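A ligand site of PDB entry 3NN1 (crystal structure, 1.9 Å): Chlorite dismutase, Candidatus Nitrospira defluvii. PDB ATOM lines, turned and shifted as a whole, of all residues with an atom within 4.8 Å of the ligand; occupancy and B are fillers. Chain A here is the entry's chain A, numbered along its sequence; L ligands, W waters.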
ATOM      1  N   PRO A 111     -15.182  24.696 -12.630  1.00  0.00           N
ATOM      2  CA  PRO A 111     -16.306  23.958 -12.024  1.00  0.00           C
ATOM      3  C   PRO A 111     -16.729  24.441 -10.649  1.00  0.00           C
ATOM      4  O   PRO A 111     -15.910  24.847  -9.827  1.00  0.00           O
ATOM      5  CB  PRO A 111     -15.805  22.514 -11.953  1.00  0.00           C
ATOM      6  CG  PRO A 111     -14.376  22.554 -12.217  1.00  0.00           C
ATOM      7  CD  PRO A 111     -14.103  23.775 -13.031  1.00  0.00           C
ATOM      8  N   THR A 112     -18.024  24.374 -10.419  1.00  0.00           N
ATOM      9  CA  THR A 112     -18.672  24.807  -9.196  1.00  0.00           C
ATOM     10  C   THR A 112     -18.771  23.700  -8.164  1.00  0.00           C
ATOM     11  O   THR A 112     -18.657  23.946  -6.956  1.00  0.00           O
ATOM     12  CB  THR A 112     -20.093  25.336  -9.542  1.00  0.00           C
ATOM     13  OG1 THR A 112     -19.949  26.513 -10.354  1.00  0.00           O
ATOM     14  CG2 THR A 112     -20.892  25.704  -8.282  1.00  0.00           C
ATOM     15  N   TYR A 113     -18.957  22.475  -8.628  1.00  0.00           N
ATOM     16  CA  TYR A 113     -19.326  21.354  -7.739  1.00  0.00           C
ATOM     17  C   TYR A 113     -18.219  20.334  -7.524  1.00  0.00           C
ATOM     18  O   TYR A 113     -18.183  19.654  -6.489  1.00  0.00           O
ATOM     19  CB  TYR A 113     -20.546  20.645  -8.322  1.00  0.00           C
ATOM     20  CG  TYR A 113     -21.754  21.539  -8.417  1.00  0.00           C
ATOM     21  CD1 TYR A 113     -22.408  21.952  -7.264  1.00  0.00           C
ATOM     22  CD2 TYR A 113     -22.219  21.995  -9.651  1.00  0.00           C
ATOM     23  CE1 TYR A 113     -23.518  22.794  -7.337  1.00  0.00           C
ATOM     24  CE2 TYR A 113     -23.331  22.803  -9.736  1.00  0.00           C
ATOM     25  CZ  TYR A 113     -23.973  23.210  -8.569  1.00  0.00           C
ATOM     26  OH  TYR A 113     -25.081  24.039  -8.648  1.00  0.00           O
ATOM     27  N   VAL A 114     -17.310  20.239  -8.492  1.00  0.00           N
ATOM     28  CA  VAL A 114     -16.322  19.144  -8.522  1.00  0.00           C
ATOM     29  C   VAL A 114     -15.449  19.116  -7.254  1.00  0.00           C
ATOM     30  O   VAL A 114     -15.089  18.038  -6.752  1.00  0.00           O
ATOM     31  CB  VAL A 114     -15.446  19.212  -9.795  1.00  0.00           C
ATOM     32  CG1 VAL A 114     -14.272  18.268  -9.708  1.00  0.00           C
ATOM     33  CG2 VAL A 114     -16.296  18.910 -11.055  1.00  0.00           C
ATOM     34  N   PHE A 117     -16.679  16.739  -4.646  1.00  0.00           N
ATOM     35  CA  PHE A 117     -16.784  15.313  -4.963  1.00  0.00           C
ATOM     36  C   PHE A 117     -15.677  14.526  -4.240  1.00  0.00           C
ATOM     37  O   PHE A 117     -14.698  15.103  -3.778  1.00  0.00           O
ATOM     38  CB  PHE A 117     -16.693  15.031  -6.477  1.00  0.00           C
ATOM     39  CG  PHE A 117     -17.799  15.658  -7.293  1.00  0.00           C
ATOM     40  CD1 PHE A 117     -18.957  16.145  -6.716  1.00  0.00           C
ATOM     41  CD2 PHE A 117     -17.664  15.741  -8.678  1.00  0.00           C
ATOM     42  CE1 PHE A 117     -19.971  16.722  -7.503  1.00  0.00           C
ATOM     43  CE2 PHE A 117     -18.670  16.290  -9.456  1.00  0.00           C
ATOM     44  CZ  PHE A 117     -19.822  16.774  -8.872  1.00  0.00           C
ATOM     45  N   LEU A 125     -12.421  12.340 -13.459  1.00  0.00           N
ATOM     46  CA  LEU A 125     -12.890  13.451 -14.315  1.00  0.00           C
ATOM     47  C   LEU A 125     -11.781  14.103 -15.132  1.00  0.00           C
ATOM     48  O   LEU A 125     -12.038  14.916 -16.022  1.00  0.00           O
ATOM     49  CB  LEU A 125     -13.629  14.510 -13.484  1.00  0.00           C
ATOM     50  CG  LEU A 125     -15.047  14.148 -13.000  1.00  0.00           C
ATOM     51  CD1 LEU A 125     -15.574  15.072 -11.883  1.00  0.00           C
ATOM     52  CD2 LEU A 125     -16.030  14.134 -14.173  1.00  0.00           C
ATOM     53  N   ILE A 140     -26.992  20.160 -26.881  1.00  0.00           N
ATOM     54  CA  ILE A 140     -28.258  20.115 -26.147  1.00  0.00           C
ATOM     55  C   ILE A 140     -28.333  21.338 -25.229  1.00  0.00           C
ATOM     56  O   ILE A 140     -27.651  21.399 -24.216  1.00  0.00           O
ATOM     57  CB  ILE A 140     -28.424  18.791 -25.351  1.00  0.00           C
ATOM     58  CG1 ILE A 140     -28.407  17.588 -26.308  1.00  0.00           C
ATOM     59  CG2 ILE A 140     -29.780  18.774 -24.602  1.00  0.00           C
ATOM     60  CD1 ILE A 140     -28.472  16.173 -25.681  1.00  0.00           C
ATOM     61  N   ILE A 142     -30.101  23.570 -22.324  1.00  0.00           N
ATOM     62  CA  ILE A 142     -30.821  23.144 -21.092  1.00  0.00           C
ATOM     63  C   ILE A 142     -31.222  24.349 -20.248  1.00  0.00           C
ATOM     64  O   ILE A 142     -30.418  25.269 -20.029  1.00  0.00           O
ATOM     65  CB  ILE A 142     -29.992  22.156 -20.263  1.00  0.00           C
ATOM     66  CG1 ILE A 142     -29.824  20.849 -21.088  1.00  0.00           C
ATOM     67  CG2 ILE A 142     -30.686  21.842 -18.899  1.00  0.00           C
ATOM     68  CD1 ILE A 142     -29.102  19.758 -20.445  1.00  0.00           C
ATOM     69  N   LYS A 144     -32.919  24.947 -16.473  1.00  0.00           N
ATOM     70  CA  LYS A 144     -33.318  24.358 -15.210  1.00  0.00           C
ATOM     71  C   LYS A 144     -34.622  24.970 -14.696  1.00  0.00           C
ATOM     72  O   LYS A 144     -35.008  26.098 -15.038  1.00  0.00           O
ATOM     73  CB  LYS A 144     -32.190  24.576 -14.172  1.00  0.00           C
ATOM     74  CG  LYS A 144     -30.930  23.854 -14.486  1.00  0.00           C
ATOM     75  CD  LYS A 144     -31.193  22.369 -14.504  1.00  0.00           C
ATOM     76  CE  LYS A 144     -30.047  21.547 -14.026  1.00  0.00           C
ATOM     77  NZ  LYS A 144     -30.424  20.121 -14.266  1.00  0.00           N
ATOM     78  N   TRP A 148     -34.629  24.012  -8.825  1.00  0.00           N
ATOM     79  CA  TRP A 148     -33.182  23.817  -8.880  1.00  0.00           C
ATOM     80  C   TRP A 148     -32.420  24.958  -8.218  1.00  0.00           C
ATOM     81  O   TRP A 148     -31.568  24.731  -7.362  1.00  0.00           O
ATOM     82  CB  TRP A 148     -32.702  23.620 -10.342  1.00  0.00           C
ATOM     83  CG  TRP A 148     -31.183  23.431 -10.464  1.00  0.00           C
ATOM     84  CD1 TRP A 148     -30.270  24.365 -10.828  1.00  0.00           C
ATOM     85  CD2 TRP A 148     -30.450  22.251 -10.171  1.00  0.00           C
ATOM     86  NE1 TRP A 148     -28.996  23.832 -10.808  1.00  0.00           N
ATOM     87  CE2 TRP A 148     -29.074  22.525 -10.405  1.00  0.00           C
ATOM     88  CE3 TRP A 148     -30.812  20.961  -9.742  1.00  0.00           C
ATOM     89  CZ2 TRP A 148     -28.072  21.572 -10.242  1.00  0.00           C
ATOM     90  CZ3 TRP A 148     -29.822  20.015  -9.580  1.00  0.00           C
ATOM     91  CH2 TRP A 148     -28.461  20.320  -9.816  1.00  0.00           C
ATOM     92  N   TRP A 149     -32.740  26.186  -8.597  1.00  0.00           N
ATOM     93  CA  TRP A 149     -32.028  27.375  -8.103  1.00  0.00           C
ATOM     94  C   TRP A 149     -32.378  27.649  -6.644  1.00  0.00           C
ATOM     95  O   TRP A 149     -31.574  28.233  -5.937  1.00  0.00           O
ATOM     96  CB  TRP A 149     -32.331  28.611  -8.984  1.00  0.00           C
ATOM     97  CG  TRP A 149     -32.073  28.365 -10.413  1.00  0.00           C
ATOM     98  CD1 TRP A 149     -32.989  28.397 -11.406  1.00  0.00           C
ATOM     99  CD2 TRP A 149     -30.822  28.032 -11.012  1.00  0.00           C
ATOM    100  NE1 TRP A 149     -32.414  28.072 -12.581  1.00  0.00           N
ATOM    101  CE2 TRP A 149     -31.072  27.868 -12.387  1.00  0.00           C
ATOM    102  CE3 TRP A 149     -29.530  27.836 -10.523  1.00  0.00           C
ATOM    103  CZ2 TRP A 149     -30.082  27.514 -13.297  1.00  0.00           C
ATOM    104  CZ3 TRP A 149     -28.529  27.487 -11.440  1.00  0.00           C
ATOM    105  CH2 TRP A 149     -28.810  27.329 -12.802  1.00  0.00           C
ATOM    106  N   MET A 160     -25.281  16.706  -8.400  1.00  0.00           N
ATOM    107  CA  MET A 160     -24.265  16.724  -9.444  1.00  0.00           C
ATOM    108  C   MET A 160     -23.257  15.586  -9.280  1.00  0.00           C
ATOM    109  O   MET A 160     -22.787  15.036 -10.267  1.00  0.00           O
ATOM    110  CB  MET A 160     -23.584  18.094  -9.568  1.00  0.00           C
ATOM    111  CG  MET A 160     -24.541  19.189 -10.068  1.00  0.00           C
ATOM    112  SD  MET A 160     -25.676  18.721 -11.415  1.00  0.00           S
ATOM    113  CE  MET A 160     -24.563  18.137 -12.713  1.00  0.00           C
ATOM    114  N   HIS A 163     -25.216  12.673 -10.885  1.00  0.00           N
ATOM    115  CA  HIS A 163     -25.024  12.940 -12.345  1.00  0.00           C
ATOM    116  C   HIS A 163     -23.697  12.373 -12.846  1.00  0.00           C
ATOM    117  O   HIS A 163     -23.650  11.586 -13.790  1.00  0.00           O
ATOM    118  CB  HIS A 163     -25.111  14.476 -12.539  1.00  0.00           C
ATOM    119  CG  HIS A 163     -24.876  14.982 -13.936  1.00  0.00           C
ATOM    120  ND1 HIS A 163     -25.913  15.457 -14.720  1.00  0.00           N
ATOM    121  CD2 HIS A 163     -23.741  15.223 -14.635  1.00  0.00           C
ATOM    122  CE1 HIS A 163     -25.425  15.931 -15.846  1.00  0.00           C
ATOM    123  NE2 HIS A 163     -24.112  15.799 -15.826  1.00  0.00           N
ATOM    124  N   THR A 164     -22.618  12.761 -12.179  1.00  0.00           N
ATOM    125  CA  THR A 164     -21.281  12.360 -12.594  1.00  0.00           C
ATOM    126  C   THR A 164     -21.113  10.848 -12.439  1.00  0.00           C
ATOM    127  O   THR A 164     -20.561  10.197 -13.318  1.00  0.00           O
ATOM    128  CB  THR A 164     -20.199  13.102 -11.771  1.00  0.00           C
ATOM    129  OG1 THR A 164     -20.427  14.510 -11.868  1.00  0.00           O
ATOM    130  CG2 THR A 164     -18.765  12.750 -12.253  1.00  0.00           C
ATOM    131  N   ALA A 167     -22.487   9.117 -15.314  1.00  0.00           N
ATOM    132  CA  ALA A 167     -21.728   9.409 -16.525  1.00  0.00           C
ATOM    133  C   ALA A 167     -20.356   8.720 -16.579  1.00  0.00           C
ATOM    134  O   ALA A 167     -19.795   8.608 -17.656  1.00  0.00           O
ATOM    135  CB  ALA A 167     -21.558  10.919 -16.690  1.00  0.00           C
ATOM    136  N   TYR A 170     -18.696   6.615 -19.402  1.00  0.00           N
ATOM    137  CA  TYR A 170     -18.650   7.213 -20.720  1.00  0.00           C
ATOM    138  C   TYR A 170     -17.543   8.260 -20.908  1.00  0.00           C
ATOM    139  O   TYR A 170     -17.459   8.875 -21.970  1.00  0.00           O
ATOM    140  CB  TYR A 170     -20.027   7.811 -21.032  1.00  0.00           C
ATOM    141  CG  TYR A 170     -21.109   6.773 -20.886  1.00  0.00           C
ATOM    142  CD1 TYR A 170     -21.408   5.900 -21.916  1.00  0.00           C
ATOM    143  CD2 TYR A 170     -21.829   6.653 -19.701  1.00  0.00           C
ATOM    144  CE1 TYR A 170     -22.393   4.922 -21.767  1.00  0.00           C
ATOM    145  CE2 TYR A 170     -22.814   5.676 -19.552  1.00  0.00           C
ATOM    146  CZ  TYR A 170     -23.078   4.818 -20.602  1.00  0.00           C
ATOM    147  OH  TYR A 170     -24.047   3.855 -20.460  1.00  0.00           O
ATOM    148  N   LEU A 171     -16.692   8.424 -19.904  1.00  0.00           N
ATOM    149  CA  LEU A 171     -15.648   9.472 -19.911  1.00  0.00           C
ATOM    150  C   LEU A 171     -14.711   9.394 -21.119  1.00  0.00           C
ATOM    151  O   LEU A 171     -14.274  10.426 -21.632  1.00  0.00           O
ATOM    152  CB  LEU A 171     -14.807   9.416 -18.644  1.00  0.00           C
ATOM    153  CG  LEU A 171     -15.450   9.915 -17.331  1.00  0.00           C
ATOM    154  CD1 LEU A 171     -14.802   9.258 -16.122  1.00  0.00           C
ATOM    155  CD2 LEU A 171     -15.333  11.424 -17.230  1.00  0.00           C
ATOM    156  N   VAL A 174     -17.076   9.603 -24.891  1.00  0.00           N
ATOM    157  CA  VAL A 174     -17.828  10.828 -25.137  1.00  0.00           C
ATOM    158  C   VAL A 174     -17.073  12.018 -24.570  1.00  0.00           C
ATOM    159  O   VAL A 174     -16.887  12.100 -23.351  1.00  0.00           O
ATOM    160  CB  VAL A 174     -19.220  10.761 -24.487  1.00  0.00           C
ATOM    161  CG1 VAL A 174     -20.000  12.081 -24.752  1.00  0.00           C
ATOM    162  CG2 VAL A 174     -19.996   9.573 -24.985  1.00  0.00           C
ATOM    163  N   ARG A 176     -16.900  15.986 -23.557  1.00  0.00           N
ATOM    164  CA  ARG A 176     -17.932  16.917 -23.055  1.00  0.00           C
ATOM    165  C   ARG A 176     -17.388  18.330 -22.884  1.00  0.00           C
ATOM    166  O   ARG A 176     -16.193  18.526 -22.572  1.00  0.00           O
ATOM    167  CB  ARG A 176     -18.455  16.441 -21.690  1.00  0.00           C
ATOM    168  CG  ARG A 176     -17.380  16.484 -20.577  1.00  0.00           C
ATOM    169  CD  ARG A 176     -17.686  15.696 -19.308  1.00  0.00           C
ATOM    170  NE  ARG A 176     -16.660  15.992 -18.293  1.00  0.00           N
ATOM    171  CZ  ARG A 176     -15.503  15.364 -18.155  1.00  0.00           C
ATOM    172  NH1 ARG A 176     -15.184  14.329 -18.919  1.00  0.00           N
ATOM    173  NH2 ARG A 176     -14.654  15.767 -17.225  1.00  0.00           N
ATOM    174  N   LEU A 178     -19.138  22.189 -21.228  1.00  0.00           N
ATOM    175  CA  LEU A 178     -20.298  22.894 -20.667  1.00  0.00           C
ATOM    176  C   LEU A 178     -20.123  24.402 -20.796  1.00  0.00           C
ATOM    177  O   LEU A 178     -19.074  24.940 -20.456  1.00  0.00           O
ATOM    178  CB  LEU A 178     -20.445  22.580 -19.167  1.00  0.00           C
ATOM    179  CG  LEU A 178     -21.618  23.157 -18.382  1.00  0.00           C
ATOM    180  CD1 LEU A 178     -22.933  22.580 -18.891  1.00  0.00           C
ATOM    181  CD2 LEU A 178     -21.490  22.911 -16.841  1.00  0.00           C
ATOM    182  N   PHE A 189     -27.785  26.560 -19.888  1.00  0.00           N
ATOM    183  CA  PHE A 189     -26.585  25.836 -20.262  1.00  0.00           C
ATOM    184  C   PHE A 189     -26.627  25.422 -21.714  1.00  0.00           C
ATOM    185  O   PHE A 189     -27.717  25.178 -22.260  1.00  0.00           O
ATOM    186  CB  PHE A 189     -26.379  24.584 -19.392  1.00  0.00           C
ATOM    187  CG  PHE A 189     -26.346  24.866 -17.920  1.00  0.00           C
ATOM    188  CD1 PHE A 189     -25.223  25.400 -17.321  1.00  0.00           C
ATOM    189  CD2 PHE A 189     -27.470  24.643 -17.143  1.00  0.00           C
ATOM    190  CE1 PHE A 189     -25.212  25.682 -15.978  1.00  0.00           C
ATOM    191  CE2 PHE A 189     -27.457  24.912 -15.807  1.00  0.00           C
ATOM    192  CZ  PHE A 189     -26.337  25.425 -15.214  1.00  0.00           C
ATOM    193  N   THR A 191     -24.787  22.365 -23.604  1.00  0.00           N
ATOM    194  CA  THR A 191     -23.935  21.186 -23.496  1.00  0.00           C
ATOM    195  C   THR A 191     -23.483  20.755 -24.886  1.00  0.00           C
ATOM    196  O   THR A 191     -24.264  20.817 -25.838  1.00  0.00           O
ATOM    197  CB  THR A 191     -24.612  20.026 -22.770  1.00  0.00           C
ATOM    198  OG1 THR A 191     -25.740  19.549 -23.528  1.00  0.00           O
ATOM    199  CG2 THR A 191     -25.075  20.485 -21.361  1.00  0.00           C
ATOM    200  N   PHE A 193     -21.057  17.764 -27.029  1.00  0.00           N
ATOM    201  CA  PHE A 193     -20.418  16.450 -26.985  1.00  0.00           C
ATOM    202  C   PHE A 193     -19.858  16.017 -28.326  1.00  0.00           C
ATOM    203  O   PHE A 193     -20.404  16.348 -29.389  1.00  0.00           O
ATOM    204  CB  PHE A 193     -21.416  15.392 -26.500  1.00  0.00           C
ATOM    205  CG  PHE A 193     -22.156  15.808 -25.253  1.00  0.00           C
ATOM    206  CD1 PHE A 193     -21.598  15.598 -24.016  1.00  0.00           C
ATOM    207  CD2 PHE A 193     -23.362  16.485 -25.346  1.00  0.00           C
ATOM    208  CE1 PHE A 193     -22.242  16.028 -22.878  1.00  0.00           C
ATOM    209  CE2 PHE A 193     -23.999  16.911 -24.214  1.00  0.00           C
ATOM    210  CZ  PHE A 193     -23.437  16.665 -22.968  1.00  0.00           C
ATOM    211  N   PHE A 201     -23.283   7.482 -26.688  1.00  0.00           N
ATOM    212  CA  PHE A 201     -23.925   8.745 -26.298  1.00  0.00           C
ATOM    213  C   PHE A 201     -25.396   8.536 -25.938  1.00  0.00           C
ATOM    214  O   PHE A 201     -25.854   9.068 -24.928  1.00  0.00           O
ATOM    215  CB  PHE A 201     -23.818   9.814 -27.392  1.00  0.00           C
ATOM    216  CG  PHE A 201     -24.404  11.127 -26.973  1.00  0.00           C
ATOM    217  CD1 PHE A 201     -23.749  11.930 -26.034  1.00  0.00           C
ATOM    218  CD2 PHE A 201     -25.609  11.582 -27.489  1.00  0.00           C
ATOM    219  CE1 PHE A 201     -24.290  13.116 -25.622  1.00  0.00           C
ATOM    220  CE2 PHE A 201     -26.156  12.772 -27.084  1.00  0.00           C
ATOM    221  CZ  PHE A 201     -25.491  13.547 -26.151  1.00  0.00           C
ATOM    222  N   LEU A 204     -25.476   6.931 -22.561  1.00  0.00           N
ATOM    223  CA  LEU A 204     -25.121   7.932 -21.561  1.00  0.00           C
ATOM    224  C   LEU A 204     -26.338   8.791 -21.173  1.00  0.00           C
ATOM    225  O   LEU A 204     -26.589   9.042 -19.999  1.00  0.00           O
ATOM    226  CB  LEU A 204     -24.010   8.837 -22.090  1.00  0.00           C
ATOM    227  CG  LEU A 204     -23.757  10.175 -21.379  1.00  0.00           C
ATOM    228  CD1 LEU A 204     -23.378   9.961 -19.939  1.00  0.00           C
ATOM    229  CD2 LEU A 204     -22.700  11.003 -22.163  1.00  0.00           C
ATOM    230  N   VAL A 205     -27.068   9.268 -22.167  1.00  0.00           N
ATOM    231  CA  VAL A 205     -28.215  10.133 -21.895  1.00  0.00           C
ATOM    232  C   VAL A 205     -29.285   9.323 -21.134  1.00  0.00           C
ATOM    233  O   VAL A 205     -29.887   9.819 -20.173  1.00  0.00           O
ATOM    234  CB  VAL A 205     -28.803  10.792 -23.151  1.00  0.00           C
ATOM    235  CG1 VAL A 205     -30.027  11.677 -22.786  1.00  0.00           C
ATOM    236  CG2 VAL A 205     -27.740  11.675 -23.824  1.00  0.00           C
ATOM    237  N   LEU A 208     -28.338   9.154 -17.511  1.00  0.00           N
ATOM    238  CA  LEU A 208     -28.627  10.411 -16.840  1.00  0.00           C
ATOM    239  C   LEU A 208     -30.118  10.688 -16.663  1.00  0.00           C
ATOM    240  O   LEU A 208     -30.485  11.432 -15.756  1.00  0.00           O
ATOM    241  CB  LEU A 208     -27.938  11.565 -17.551  1.00  0.00           C
ATOM    242  CG  LEU A 208     -26.418  11.605 -17.434  1.00  0.00           C
ATOM    243  CD1 LEU A 208     -25.818  12.601 -18.434  1.00  0.00           C
ATOM    244  CD2 LEU A 208     -25.985  11.932 -16.014  1.00  0.00           C
ATOM    245  N   GLU A 213     -31.324  14.935 -10.684  1.00  0.00           N
ATOM    246  CA  GLU A 213     -31.058  16.206 -11.379  1.00  0.00           C
ATOM    247  C   GLU A 213     -31.829  16.349 -12.731  1.00  0.00           C
ATOM    248  O   GLU A 213     -32.221  17.445 -13.122  1.00  0.00           O
ATOM    249  CB  GLU A 213     -29.541  16.335 -11.635  1.00  0.00           C
ATOM    250  CG  GLU A 213     -29.062  17.569 -12.417  1.00  0.00           C
ATOM    251  CD  GLU A 213     -28.654  17.320 -13.845  1.00  0.00           C
ATOM    252  OE1 GLU A 213     -28.462  16.131 -14.240  1.00  0.00           O
ATOM    253  OE2 GLU A 213     -28.459  18.333 -14.591  1.00  0.00           O
ATOM    254  N   PHE A 220     -35.083  20.769 -22.277  1.00  0.00           N
ATOM    255  CA  PHE A 220     -33.973  19.901 -22.600  1.00  0.00           C
ATOM    256  C   PHE A 220     -34.074  19.723 -24.122  1.00  0.00           C
ATOM    257  O   PHE A 220     -35.089  19.211 -24.610  1.00  0.00           O
ATOM    258  CB  PHE A 220     -34.172  18.583 -21.856  1.00  0.00           C
ATOM    259  CG  PHE A 220     -33.033  17.633 -21.983  1.00  0.00           C
ATOM    260  CD1 PHE A 220     -32.003  17.641 -21.049  1.00  0.00           C
ATOM    261  CD2 PHE A 220     -32.988  16.710 -23.007  1.00  0.00           C
ATOM    262  CE1 PHE A 220     -30.985  16.745 -21.113  1.00  0.00           C
ATOM    263  CE2 PHE A 220     -31.956  15.795 -23.077  1.00  0.00           C
ATOM    264  CZ  PHE A 220     -30.939  15.822 -22.151  1.00  0.00           C
HETATM  265  C1  LIG L   1     -22.666  19.629 -15.257  1.00  0.00           C
HETATM  266  C2  LIG L   1     -20.087  15.606 -15.629  1.00  0.00           C
HETATM  267  C3  LIG L   1     -22.782  14.400 -19.433  1.00  0.00           C
HETATM  268  C4  LIG L   1     -25.813  18.060 -18.568  1.00  0.00           C
HETATM  269  C5  LIG L   1     -21.746  18.653 -15.012  1.00  0.00           C
HETATM  270  C6  LIG L   1     -20.769  18.669 -13.967  1.00  0.00           C
HETATM  271  C7  LIG L   1     -20.037  17.564 -14.082  1.00  0.00           C
HETATM  272  C8  LIG L   1     -20.555  16.809 -15.199  1.00  0.00           C
HETATM  273  C9  LIG L   1     -18.849  17.099 -13.198  1.00  0.00           C
HETATM  274  C10 LIG L   1     -20.558  19.772 -12.894  1.00  0.00           C
HETATM  275  C11 LIG L   1     -19.617  20.860 -13.376  1.00  0.00           C
HETATM  276  C12 LIG L   1     -19.381  21.893 -12.299  1.00  0.00           C
HETATM  277  O1  LIG L   1     -18.990  21.476 -11.177  1.00  0.00           O
HETATM  278  O2  LIG L   1     -19.577  23.135 -12.516  1.00  0.00           O
HETATM  279  C13 LIG L   1     -20.526  14.979 -16.768  1.00  0.00           C
HETATM  280  C14 LIG L   1     -19.846  13.907 -17.454  1.00  0.00           C
HETATM  281  C15 LIG L   1     -20.586  13.581 -18.530  1.00  0.00           C
HETATM  282  C16 LIG L   1     -21.754  14.443 -18.536  1.00  0.00           C
HETATM  283  C17 LIG L   1     -18.503  13.320 -16.939  1.00  0.00           C
HETATM  284  C18 LIG L   1     -20.350  12.508 -19.643  1.00  0.00           C
HETATM  285  C19 LIG L   1     -19.234  11.797 -19.774  1.00  0.00           C
HETATM  286  C20 LIG L   1     -23.894  15.243 -19.478  1.00  0.00           C
HETATM  287  C21 LIG L   1     -24.976  15.138 -20.411  1.00  0.00           C
HETATM  288  C22 LIG L   1     -25.804  16.171 -20.171  1.00  0.00           C
HETATM  289  C23 LIG L   1     -25.262  16.935 -19.095  1.00  0.00           C
HETATM  290  C24 LIG L   1     -25.145  14.023 -21.481  1.00  0.00           C
HETATM  291  C25 LIG L   1     -27.120  16.549 -20.846  1.00  0.00           C
HETATM  292  C26 LIG L   1     -27.321  16.382 -22.154  1.00  0.00           C
HETATM  293  C27 LIG L   1     -25.196  18.850 -17.645  1.00  0.00           C
HETATM  294  C28 LIG L   1     -25.735  20.103 -17.207  1.00  0.00           C
HETATM  295  C29 LIG L   1     -24.737  20.596 -16.209  1.00  0.00           C
HETATM  296  C30 LIG L   1     -23.736  19.575 -16.099  1.00  0.00           C
HETATM  297  C31 LIG L   1     -27.021  20.751 -17.728  1.00  0.00           C
HETATM  298  C32 LIG L   1     -24.790  21.919 -15.400  1.00  0.00           C
HETATM  299  C33 LIG L   1     -25.612  21.696 -14.139  1.00  0.00           C
HETATM  300  C34 LIG L   1     -25.374  22.818 -13.186  1.00  0.00           C
HETATM  301  O3  LIG L   1     -24.196  23.215 -13.017  1.00  0.00           O
HETATM  302  O4  LIG L   1     -26.373  23.321 -12.580  1.00  0.00           O
HETATM  303  N1  LIG L   1     -21.638  17.471 -15.752  1.00  0.00           N
HETATM  304  N2  LIG L   1     -21.701  15.291 -17.433  1.00  0.00           N
HETATM  305  N3  LIG L   1     -24.095  16.351 -18.683  1.00  0.00           N
HETATM  306  N4  LIG L   1     -24.028  18.541 -16.974  1.00  0.00           N
HETATM  307 FE1  LIG L   1     -22.873  16.853 -17.176  1.00  0.00          FE
HETATM  308  O   HOH W   1     -16.218  12.867 -20.950  1.00  0.00           O
HETATM  309  O   HOH W   2     -21.970  24.511 -12.906  1.00  0.00           O
HETATM  310  O   HOH W   3     -18.842  24.442 -14.768  1.00  0.00           O
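FE1 of the ligand is bound by NE2 of His 163, 2.1 Å away.
NE1 of Trp 148 sits at hydrogen-bond distance from O4 of the ligand, at 3.2 Å.
The backbone NH (N) of Val 114 lies within hydrogen-bond range of an oxygen (O1) of the ligand (3.4 Å).
N of Tyr 113 lies within hydrogen-bond range of O1 of the ligand (2.7 Å).
N of Thr 112 is in hydrogen-bond range of O2 of the ligand (2.9 Å).
The guanidinium group (NH2) of Arg 176 sits at hydrogen-bond distance from the backbone carbonyl oxygen (O) of Leu 125 (3.0 Å).
The backbone carbonyl oxygen (O) of Phe 189 lies within hydrogen-bond range of the backbone NH (N) of Ile 142, at 2.9 Å.
The backbone carbonyl oxygen (O) of Ile 140 lies within hydrogen-bond range of the side-chain hydroxyl (OG1) of Thr 191.
ND1 of His 163 lies within hydrogen-bond range of OE1 of Glu 213 (2.7 Å).
The backbone carbonyl oxygen (O) of Met 160 sits at hydrogen-bond distance from the side-chain hydroxyl (OG1) of Thr 164, 2.9 Å away.
Merely in contact with the ligand: Thr 164, Leu 208, Phe 193, Arg 176, Phe 189, Ala 167, Pro 111, Met 160, Ile 142, Phe 220, Leu 171, Ile 140, Leu 178, Leu 204, Thr 191, Leu 125 and Phe 117.
Hydrophobic or aromatic side chains that line the ligand: Pro 111, Tyr 113, Val 114, Phe 117, Leu 125, Ile 140, Ile 142, Trp 148, Met 160, His 163, Ala 167, Leu 171, Leu 178, Phe 189, Phe 193, Leu 204, Leu 208 and Phe 220.
22 residues have an atom within 4 Å of the ligand: Pro 111, Thr 112, Tyr 113, Val 114, Phe 117, Leu 125, Ile 140, Ile 142, Trp 148, Met 160, His 163, Thr 164, Ala 167, Leu 171, Arg 176, Leu 178, Phe 189, Thr 191, Phe 193, Leu 204, Leu 208 and Phe 220.
Along chain A the residues within 4 Å of the ligand span positions 111 to 220.
Water W1 lies within hydrogen-bond range of O of Val 174, NH1 of Arg 176 and O of Leu 171.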
